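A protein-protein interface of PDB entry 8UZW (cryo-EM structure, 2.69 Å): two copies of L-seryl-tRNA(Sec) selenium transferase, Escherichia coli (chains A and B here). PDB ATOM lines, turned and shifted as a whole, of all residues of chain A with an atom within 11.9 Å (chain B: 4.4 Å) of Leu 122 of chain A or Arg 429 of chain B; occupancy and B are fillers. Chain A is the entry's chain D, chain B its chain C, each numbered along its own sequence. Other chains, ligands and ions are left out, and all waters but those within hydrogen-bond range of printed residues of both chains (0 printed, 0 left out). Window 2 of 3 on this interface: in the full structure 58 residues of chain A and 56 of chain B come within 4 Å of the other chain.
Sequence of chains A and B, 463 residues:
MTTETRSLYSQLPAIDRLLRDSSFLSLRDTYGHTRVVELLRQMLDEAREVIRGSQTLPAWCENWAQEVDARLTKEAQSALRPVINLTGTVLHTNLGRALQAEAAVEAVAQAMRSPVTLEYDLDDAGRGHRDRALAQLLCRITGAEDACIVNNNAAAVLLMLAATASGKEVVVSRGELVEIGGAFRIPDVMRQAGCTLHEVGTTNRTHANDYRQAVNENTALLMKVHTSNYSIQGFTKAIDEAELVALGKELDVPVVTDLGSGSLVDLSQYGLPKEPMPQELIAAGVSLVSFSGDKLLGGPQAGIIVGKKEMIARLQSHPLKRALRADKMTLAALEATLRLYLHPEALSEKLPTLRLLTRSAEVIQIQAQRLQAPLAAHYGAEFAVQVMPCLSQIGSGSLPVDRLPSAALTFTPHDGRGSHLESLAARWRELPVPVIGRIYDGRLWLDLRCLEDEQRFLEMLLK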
ATOM      1  N   GLN A 110       2.305 -31.711 -15.545  1.00  0.00           N
ATOM      2  CA  GLN A 110       3.603 -31.858 -14.898  1.00  0.00           C
ATOM      3  C   GLN A 110       4.049 -30.561 -14.237  1.00  0.00           C
ATOM      4  O   GLN A 110       4.523 -30.569 -13.096  1.00  0.00           O
ATOM      5  CB  GLN A 110       4.634 -32.327 -15.924  1.00  0.00           C
ATOM      6  CG  GLN A 110       6.045 -31.842 -15.668  1.00  0.00           C
ATOM      7  CD  GLN A 110       6.807 -31.593 -16.951  1.00  0.00           C
ATOM      8  OE1 GLN A 110       7.133 -32.528 -17.683  1.00  0.00           O
ATOM      9  NE2 GLN A 110       7.092 -30.328 -17.236  1.00  0.00           N
ATOM     10  N   PRO A 115       6.888 -28.201  -8.645  1.00  0.00           N
ATOM     11  CA  PRO A 115       7.560 -26.922  -8.905  1.00  0.00           C
ATOM     12  C   PRO A 115       8.383 -26.983 -10.182  1.00  0.00           C
ATOM     13  O   PRO A 115       8.948 -28.020 -10.530  1.00  0.00           O
ATOM     14  CB  PRO A 115       8.450 -26.729  -7.671  1.00  0.00           C
ATOM     15  CG  PRO A 115       7.913 -27.658  -6.642  1.00  0.00           C
ATOM     16  CD  PRO A 115       7.343 -28.815  -7.387  1.00  0.00           C
ATOM     17  N   VAL A 116       8.442 -25.855 -10.888  1.00  0.00           N
ATOM     18  CA  VAL A 116       9.197 -25.755 -12.128  1.00  0.00           C
ATOM     19  C   VAL A 116      10.036 -24.487 -12.098  1.00  0.00           C
ATOM     20  O   VAL A 116       9.727 -23.524 -11.396  1.00  0.00           O
ATOM     21  CB  VAL A 116       8.284 -25.761 -13.372  1.00  0.00           C
ATOM     22  CG1 VAL A 116       7.685 -27.140 -13.577  1.00  0.00           C
ATOM     23  CG2 VAL A 116       7.198 -24.713 -13.233  1.00  0.00           C
ATOM     24  N   THR A 117      11.107 -24.494 -12.889  1.00  0.00           N
ATOM     25  CA  THR A 117      11.995 -23.342 -12.964  1.00  0.00           C
ATOM     26  C   THR A 117      11.344 -22.224 -13.769  1.00  0.00           C
ATOM     27  O   THR A 117      11.760 -21.936 -14.896  1.00  0.00           O
ATOM     28  CB  THR A 117      13.335 -23.735 -13.585  1.00  0.00           C
ATOM     29  OG1 THR A 117      13.107 -24.577 -14.723  1.00  0.00           O
ATOM     30  CG2 THR A 117      14.185 -24.482 -12.571  1.00  0.00           C
ATOM     31  N   LEU A 118      10.318 -21.597 -13.193  1.00  0.00           N
ATOM     32  CA  LEU A 118       9.591 -20.547 -13.897  1.00  0.00           C
ATOM     33  C   LEU A 118      10.452 -19.301 -14.070  1.00  0.00           C
ATOM     34  O   LEU A 118      10.534 -18.738 -15.167  1.00  0.00           O
ATOM     35  CB  LEU A 118       8.305 -20.218 -13.140  1.00  0.00           C
ATOM     36  CG  LEU A 118       7.376 -19.160 -13.731  1.00  0.00           C
ATOM     37  CD1 LEU A 118       7.040 -19.495 -15.169  1.00  0.00           C
ATOM     38  CD2 LEU A 118       6.117 -19.055 -12.893  1.00  0.00           C
ATOM     39  N   GLU A 119      11.100 -18.857 -12.995  1.00  0.00           N
ATOM     40  CA  GLU A 119      11.946 -17.671 -13.021  1.00  0.00           C
ATOM     41  C   GLU A 119      13.281 -17.949 -12.339  1.00  0.00           C
ATOM     42  O   GLU A 119      13.909 -17.039 -11.791  1.00  0.00           O
ATOM     43  CB  GLU A 119      11.239 -16.486 -12.366  1.00  0.00           C
ATOM     44  CG  GLU A 119      11.594 -15.135 -12.959  1.00  0.00           C
ATOM     45  CD  GLU A 119      10.736 -14.016 -12.402  1.00  0.00           C
ATOM     46  OE1 GLU A 119       9.922 -14.286 -11.495  1.00  0.00           O
ATOM     47  OE2 GLU A 119      10.875 -12.868 -12.872  1.00  0.00           O
ATOM     48  N   TYR A 120      13.716 -19.206 -12.359  1.00  0.00           N
ATOM     49  CA  TYR A 120      14.965 -19.631 -11.742  1.00  0.00           C
ATOM     50  C   TYR A 120      15.871 -20.199 -12.824  1.00  0.00           C
ATOM     51  O   TYR A 120      15.506 -21.169 -13.496  1.00  0.00           O
ATOM     52  CB  TYR A 120      14.708 -20.674 -10.651  1.00  0.00           C
ATOM     53  CG  TYR A 120      15.862 -20.863  -9.693  1.00  0.00           C
ATOM     54  CD1 TYR A 120      15.969 -20.091  -8.544  1.00  0.00           C
ATOM     55  CD2 TYR A 120      16.840 -21.818  -9.935  1.00  0.00           C
ATOM     56  CE1 TYR A 120      17.021 -20.263  -7.667  1.00  0.00           C
ATOM     57  CE2 TYR A 120      17.895 -21.995  -9.064  1.00  0.00           C
ATOM     58  CZ  TYR A 120      17.981 -21.215  -7.931  1.00  0.00           C
ATOM     59  OH  TYR A 120      19.031 -21.389  -7.059  1.00  0.00           O
ATOM     60  N   ASP A 121      17.048 -19.601 -12.984  1.00  0.00           N
ATOM     61  CA  ASP A 121      18.005 -20.039 -13.991  1.00  0.00           C
ATOM     62  C   ASP A 121      18.978 -21.034 -13.373  1.00  0.00           C
ATOM     63  O   ASP A 121      19.453 -20.834 -12.250  1.00  0.00           O
ATOM     64  CB  ASP A 121      18.763 -18.850 -14.578  1.00  0.00           C
ATOM     65  CG  ASP A 121      19.159 -19.069 -16.023  1.00  0.00           C
ATOM     66  OD1 ASP A 121      19.497 -20.217 -16.379  1.00  0.00           O
ATOM     67  OD2 ASP A 121      19.129 -18.096 -16.805  1.00  0.00           O
ATOM     68  N   LEU A 122      19.267 -22.105 -14.105  1.00  0.00           N
ATOM     69  CA  LEU A 122      20.134 -23.163 -13.604  1.00  0.00           C
ATOM     70  C   LEU A 122      21.536 -23.057 -14.195  1.00  0.00           C
ATOM     71  O   LEU A 122      22.431 -22.465 -13.592  1.00  0.00           O
ATOM     72  CB  LEU A 122      19.531 -24.532 -13.917  1.00  0.00           C
ATOM     73  CG  LEU A 122      18.159 -24.800 -13.293  1.00  0.00           C
ATOM     74  CD1 LEU A 122      17.545 -26.063 -13.869  1.00  0.00           C
ATOM     75  CD2 LEU A 122      18.260 -24.890 -11.779  1.00  0.00           C
ATOM     76  N   ARG A 127      19.008 -14.825 -11.229  1.00  0.00           N
ATOM     77  CA  ARG A 127      17.727 -15.301 -11.735  1.00  0.00           C
ATOM     78  C   ARG A 127      17.643 -15.155 -13.251  1.00  0.00           C
ATOM     79  O   ARG A 127      18.231 -14.242 -13.834  1.00  0.00           O
ATOM     80  CB  ARG A 127      16.575 -14.545 -11.067  1.00  0.00           C
ATOM     81  CG  ARG A 127      16.487 -13.075 -11.449  1.00  0.00           C
ATOM     82  CD  ARG A 127      15.328 -12.378 -10.755  1.00  0.00           C
ATOM     83  NE  ARG A 127      15.515 -12.313  -9.311  1.00  0.00           N
ATOM     84  CZ  ARG A 127      14.731 -12.913  -8.424  1.00  0.00           C
ATOM     85  NH1 ARG A 127      13.675 -13.616  -8.800  1.00  0.00           N
ATOM     86  NH2 ARG A 127      15.013 -12.802  -7.130  1.00  0.00           N
ATOM     87  N   GLY A 128      16.914 -16.067 -13.887  1.00  0.00           N
ATOM     88  CA  GLY A 128      16.690 -16.034 -15.321  1.00  0.00           C
ATOM     89  C   GLY A 128      15.293 -15.528 -15.624  1.00  0.00           C
ATOM     90  O   GLY A 128      14.402 -15.586 -14.774  1.00  0.00           O
ATOM     91  N   HIS A 129      15.105 -15.025 -16.840  1.00  0.00           N
ATOM     92  CA  HIS A 129      13.817 -14.453 -17.195  1.00  0.00           C
ATOM     93  C   HIS A 129      12.777 -15.555 -17.392  1.00  0.00           C
ATOM     94  O   HIS A 129      13.097 -16.732 -17.575  1.00  0.00           O
ATOM     95  CB  HIS A 129      13.934 -13.586 -18.448  1.00  0.00           C
ATOM     96  CG  HIS A 129      12.783 -12.647 -18.640  1.00  0.00           C
ATOM     97  ND1 HIS A 129      11.577 -13.043 -19.178  1.00  0.00           N
ATOM     98  CD2 HIS A 129      12.650 -11.331 -18.349  1.00  0.00           C
ATOM     99  CE1 HIS A 129      10.753 -12.011 -19.215  1.00  0.00           C
ATOM    100  NE2 HIS A 129      11.380 -10.960 -18.719  1.00  0.00           N
ATOM    101  N   ARG A 130      11.510 -15.142 -17.346  1.00  0.00           N
ATOM    102  CA  ARG A 130      10.403 -16.090 -17.288  1.00  0.00           C
ATOM    103  C   ARG A 130      10.246 -16.876 -18.587  1.00  0.00           C
ATOM    104  O   ARG A 130       9.953 -18.077 -18.558  1.00  0.00           O
ATOM    105  CB  ARG A 130       9.116 -15.340 -16.950  1.00  0.00           C
ATOM    106  CG  ARG A 130       7.922 -16.227 -16.717  1.00  0.00           C
ATOM    107  CD  ARG A 130       6.734 -15.435 -16.209  1.00  0.00           C
ATOM    108  NE  ARG A 130       6.649 -15.472 -14.756  1.00  0.00           N
ATOM    109  CZ  ARG A 130       5.519 -15.606 -14.078  1.00  0.00           C
ATOM    110  NH1 ARG A 130       4.356 -15.726 -14.691  1.00  0.00           N
ATOM    111  NH2 ARG A 130       5.560 -15.626 -12.750  1.00  0.00           N
ATOM    112  N   ARG A 132      12.419 -17.174 -21.528  1.00  0.00           N
ATOM    113  CA  ARG A 132      13.558 -17.301 -22.433  1.00  0.00           C
ATOM    114  C   ARG A 132      13.531 -18.590 -23.247  1.00  0.00           C
ATOM    115  O   ARG A 132      13.931 -18.581 -24.416  1.00  0.00           O
ATOM    116  CB  ARG A 132      14.870 -17.194 -21.657  1.00  0.00           C
ATOM    117  CG  ARG A 132      15.068 -15.855 -20.969  1.00  0.00           C
ATOM    118  CD  ARG A 132      15.540 -14.788 -21.958  1.00  0.00           C
ATOM    119  NE  ARG A 132      14.482 -14.339 -22.857  1.00  0.00           N
ATOM    120  CZ  ARG A 132      13.670 -13.320 -22.618  1.00  0.00           C
ATOM    121  NH1 ARG A 132      13.788 -12.583 -21.528  1.00  0.00           N
ATOM    122  NH2 ARG A 132      12.719 -13.027 -23.500  1.00  0.00           N
ATOM    123  N   ALA A 133      13.080 -19.700 -22.659  1.00  0.00           N
ATOM    124  CA  ALA A 133      12.972 -20.937 -23.426  1.00  0.00           C
ATOM    125  C   ALA A 133      11.994 -20.777 -24.580  1.00  0.00           C
ATOM    126  O   ALA A 133      12.264 -21.210 -25.707  1.00  0.00           O
ATOM    127  CB  ALA A 133      12.540 -22.083 -22.517  1.00  0.00           C
ATOM    128  N   ARG B  81      11.867 -27.238 -16.277  1.00  0.00           N
ATOM    129  CA  ARG B  81      12.079 -28.562 -15.709  1.00  0.00           C
ATOM    130  C   ARG B  81      11.379 -28.676 -14.361  1.00  0.00           C
ATOM    131  O   ARG B  81      11.403 -27.722 -13.575  1.00  0.00           O
ATOM    132  CB  ARG B  81      13.574 -28.822 -15.539  1.00  0.00           C
ATOM    133  CG  ARG B  81      14.421 -28.300 -16.683  1.00  0.00           C
ATOM    134  CD  ARG B  81      15.898 -28.289 -16.334  1.00  0.00           C
ATOM    135  NE  ARG B  81      16.546 -29.566 -16.603  1.00  0.00           N
ATOM    136  CZ  ARG B  81      17.831 -29.810 -16.391  1.00  0.00           C
ATOM    137  NH1 ARG B  81      18.637 -28.887 -15.891  1.00  0.00           N
ATOM    138  NH2 ARG B  81      18.322 -31.010 -16.687  1.00  0.00           N
ATOM    139  N   ALA B 425      26.330 -28.371  -6.144  1.00  0.00           N
ATOM    140  CA  ALA B 425      25.174 -27.609  -6.605  1.00  0.00           C
ATOM    141  C   ALA B 425      25.088 -27.605  -8.126  1.00  0.00           C
ATOM    142  O   ALA B 425      23.998 -27.743  -8.693  1.00  0.00           O
ATOM    143  CB  ALA B 425      25.238 -26.181  -6.065  1.00  0.00           C
ATOM    144  N   ALA B 426      26.229 -27.448  -8.803  1.00  0.00           N
ATOM    145  CA  ALA B 426      26.235 -27.495 -10.262  1.00  0.00           C
ATOM    146  C   ALA B 426      25.839 -28.874 -10.774  1.00  0.00           C
ATOM    147  O   ALA B 426      25.132 -28.990 -11.781  1.00  0.00           O
ATOM    148  CB  ALA B 426      27.612 -27.101 -10.795  1.00  0.00           C
ATOM    149  N   ARG B 427      26.296 -29.931 -10.098  1.00  0.00           N
ATOM    150  CA  ARG B 427      25.921 -31.286 -10.484  1.00  0.00           C
ATOM    151  C   ARG B 427      24.421 -31.502 -10.349  1.00  0.00           C
ATOM    152  O   ARG B 427      23.793 -32.123 -11.214  1.00  0.00           O
ATOM    153  CB  ARG B 427      26.678 -32.302  -9.627  1.00  0.00           C
ATOM    154  CG  ARG B 427      27.842 -32.984 -10.321  1.00  0.00           C
ATOM    155  CD  ARG B 427      28.661 -33.779  -9.317  1.00  0.00           C
ATOM    156  NE  ARG B 427      27.881 -34.858  -8.723  1.00  0.00           N
ATOM    157  CZ  ARG B 427      28.259 -35.564  -7.666  1.00  0.00           C
ATOM    158  NH1 ARG B 427      29.412 -35.335  -7.058  1.00  0.00           N
ATOM    159  NH2 ARG B 427      27.460 -36.522  -7.205  1.00  0.00           N
ATOM    160  N   TRP B 428      23.830 -31.003  -9.263  1.00  0.00           N
ATOM    161  CA  TRP B 428      22.402 -31.208  -9.048  1.00  0.00           C
ATOM    162  C   TRP B 428      21.565 -30.359  -9.998  1.00  0.00           C
ATOM    163  O   TRP B 428      20.523 -30.812 -10.487  1.00  0.00           O
ATOM    164  CB  TRP B 428      22.047 -30.912  -7.592  1.00  0.00           C
ATOM    165  CG  TRP B 428      22.555 -31.959  -6.656  1.00  0.00           C
ATOM    166  CD1 TRP B 428      23.056 -33.182  -6.992  1.00  0.00           C
ATOM    167  CD2 TRP B 428      22.616 -31.879  -5.229  1.00  0.00           C
ATOM    168  NE1 TRP B 428      23.424 -33.871  -5.863  1.00  0.00           N
ATOM    169  CE2 TRP B 428      23.165 -33.092  -4.767  1.00  0.00           C
ATOM    170  CE3 TRP B 428      22.262 -30.901  -4.297  1.00  0.00           C
ATOM    171  CZ2 TRP B 428      23.366 -33.352  -3.415  1.00  0.00           C
ATOM    172  CZ3 TRP B 428      22.461 -31.162  -2.955  1.00  0.00           C
ATOM    173  CH2 TRP B 428      23.009 -32.377  -2.527  1.00  0.00           C
ATOM    174  N   ARG B 429      22.004 -29.130 -10.279  1.00  0.00           N
ATOM    175  CA  ARG B 429      21.244 -28.259 -11.169  1.00  0.00           C
ATOM    176  C   ARG B 429      21.260 -28.743 -12.614  1.00  0.00           C
ATOM    177  O   ARG B 429      20.446 -28.277 -13.418  1.00  0.00           O
ATOM    178  CB  ARG B 429      21.778 -26.827 -11.086  1.00  0.00           C
ATOM    179  CG  ARG B 429      21.353 -26.094  -9.825  1.00  0.00           C
ATOM    180  CD  ARG B 429      21.780 -24.633  -9.831  1.00  0.00           C
ATOM    181  NE  ARG B 429      23.107 -24.443  -9.255  1.00  0.00           N
ATOM    182  CZ  ARG B 429      24.074 -23.732  -9.817  1.00  0.00           C
ATOM    183  NH1 ARG B 429      23.901 -23.125 -10.979  1.00  0.00           N
ATOM    184  NH2 ARG B 429      25.245 -23.627  -9.195  1.00  0.00           N
ATOM    185  N   GLU B 430      22.163 -29.656 -12.963  1.00  0.00           N
ATOM    186  CA  GLU B 430      22.240 -30.203 -14.310  1.00  0.00           C
ATOM    187  C   GLU B 430      21.443 -31.490 -14.480  1.00  0.00           C
ATOM    188  O   GLU B 430      21.353 -32.000 -15.601  1.00  0.00           O
ATOM    189  CB  GLU B 430      23.703 -30.454 -14.690  1.00  0.00           C
ATOM    190  N   LEU B 431      20.862 -32.021 -13.407  1.00  0.00           N
ATOM    191  CA  LEU B 431      20.123 -33.270 -13.496  1.00  0.00           C
ATOM    192  C   LEU B 431      18.815 -33.065 -14.260  1.00  0.00           C
ATOM    193  O   LEU B 431      18.290 -31.949 -14.317  1.00  0.00           O
ATOM    194  CB  LEU B 431      19.829 -33.813 -12.100  1.00  0.00           C
ATOM    195  CG  LEU B 431      21.039 -34.158 -11.233  1.00  0.00           C
ATOM    196  CD1 LEU B 431      20.608 -34.471  -9.810  1.00  0.00           C
ATOM    197  CD2 LEU B 431      21.813 -35.320 -11.832  1.00  0.00           C
ATOM    198  N   PRO B 434      16.136 -31.344 -11.504  1.00  0.00           N
ATOM    199  CA  PRO B 434      17.108 -30.696 -10.617  1.00  0.00           C
ATOM    200  C   PRO B 434      16.641 -30.667  -9.171  1.00  0.00           C
ATOM    201  O   PRO B 434      15.445 -30.641  -8.876  1.00  0.00           O
ATOM    202  CB  PRO B 434      17.222 -29.278 -11.191  1.00  0.00           C
ATOM    203  CG  PRO B 434      16.746 -29.395 -12.596  1.00  0.00           C
ATOM    204  CD  PRO B 434      15.685 -30.446 -12.578  1.00  0.00           C
ATOM    205  N   ILE B 436      17.318 -28.390  -5.739  1.00  0.00           N
ATOM    206  CA  ILE B 436      17.815 -27.082  -5.331  1.00  0.00           C
ATOM    207  C   ILE B 436      17.889 -27.057  -3.811  1.00  0.00           C
ATOM    208  O   ILE B 436      16.886 -27.298  -3.128  1.00  0.00           O
ATOM    209  CB  ILE B 436      16.926 -25.947  -5.859  1.00  0.00           C
ATOM    210  CG1 ILE B 436      16.933 -25.931  -7.386  1.00  0.00           C
ATOM    211  CG2 ILE B 436      17.422 -24.608  -5.351  1.00  0.00           C
ATOM    212  CD1 ILE B 436      18.306 -26.022  -7.985  1.00  0.00           C
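O of Arg 81 of chain B lies within hydrogen-bond range of N of Thr 117 of chain A. The guanidinium group of Arg 429 of chain B sits at hydrogen-bond distance from the backbone carbonyl oxygen of Leu 122 of chain A (3.1 Å).
NH1 of Arg 81 of chain B sits at hydrogen-bond distance from O of Arg 429 of chain B (3.1 Å). NH2 of Arg 81 of chain B lies within hydrogen-bond range of O of Glu 430 of chain B, 3.4 Å away. NH2 of Arg 81 of chain B sits at hydrogen-bond distance from O of Leu 431 of chain B (2.5 Å). O of Ala 425 of chain B sits close to NE of Arg 429 of chain B (3.5 Å).
Among the printed residues, merely in contact across the chains: Pro 115 of chain A with Arg 81 of chain B (3.9 Å), Val 116 of chain A with Arg 81 of chain B (3.3 Å), Tyr 120 of chain A with Ile 436 of chain B (3.98 Å), Leu 122 of chain A with Arg 81 of chain B (3.6 Å), Leu 122 of chain A with Pro 434 of chain B (3.7 Å) and Leu 122 of chain A with Ile 436 of chain B (3.96 Å).
Leu 122 of chain A touches just these residues of chain B: Arg 81 (3.6 Å), Arg 429 (3.1 Å), Pro 434 (3.7 Å) and Ile 436 (3.96 Å). Arg 429 of chain B touches just one residue of chain A: Leu 122 (3.1 Å). No residue of chain A comes within 4 Å of Ala 425 of chain B. Ala 426 of chain B touches none of the printed residues of chain A. Leu 431 of chain B touches none of the printed residues of chain A. Of the printed residues of chain B, Pro 115 of chain A touches Arg 81. Of the printed residues of chain B, Val 116 of chain A touches Arg 81. Printed residues of chain A within 4 Å of Ile 436 of chain B: Tyr 120 and Leu 122. The nearest residue of chain A that does not touch Arg 429 of chain B is Tyr 120 of chain A (4.8 Å). The nearest printed residue of chain B that does not touch Pro 115 of chain A is Pro 434 of chain B (7.2 Å).
Of the 15 printed residues of chain A, 5 touch a printed residue of chain B. Hydrophobic or aromatic side chains of chain B that line the printed part of chain A: Pro 434 and Ile 436. Among the printed residues, 8 pairs touch across the chains.
No position is printed for both chains. Of the 8 pairs that touch across the chains among the printed residues, none has its exchanged pair printed and touching as well.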
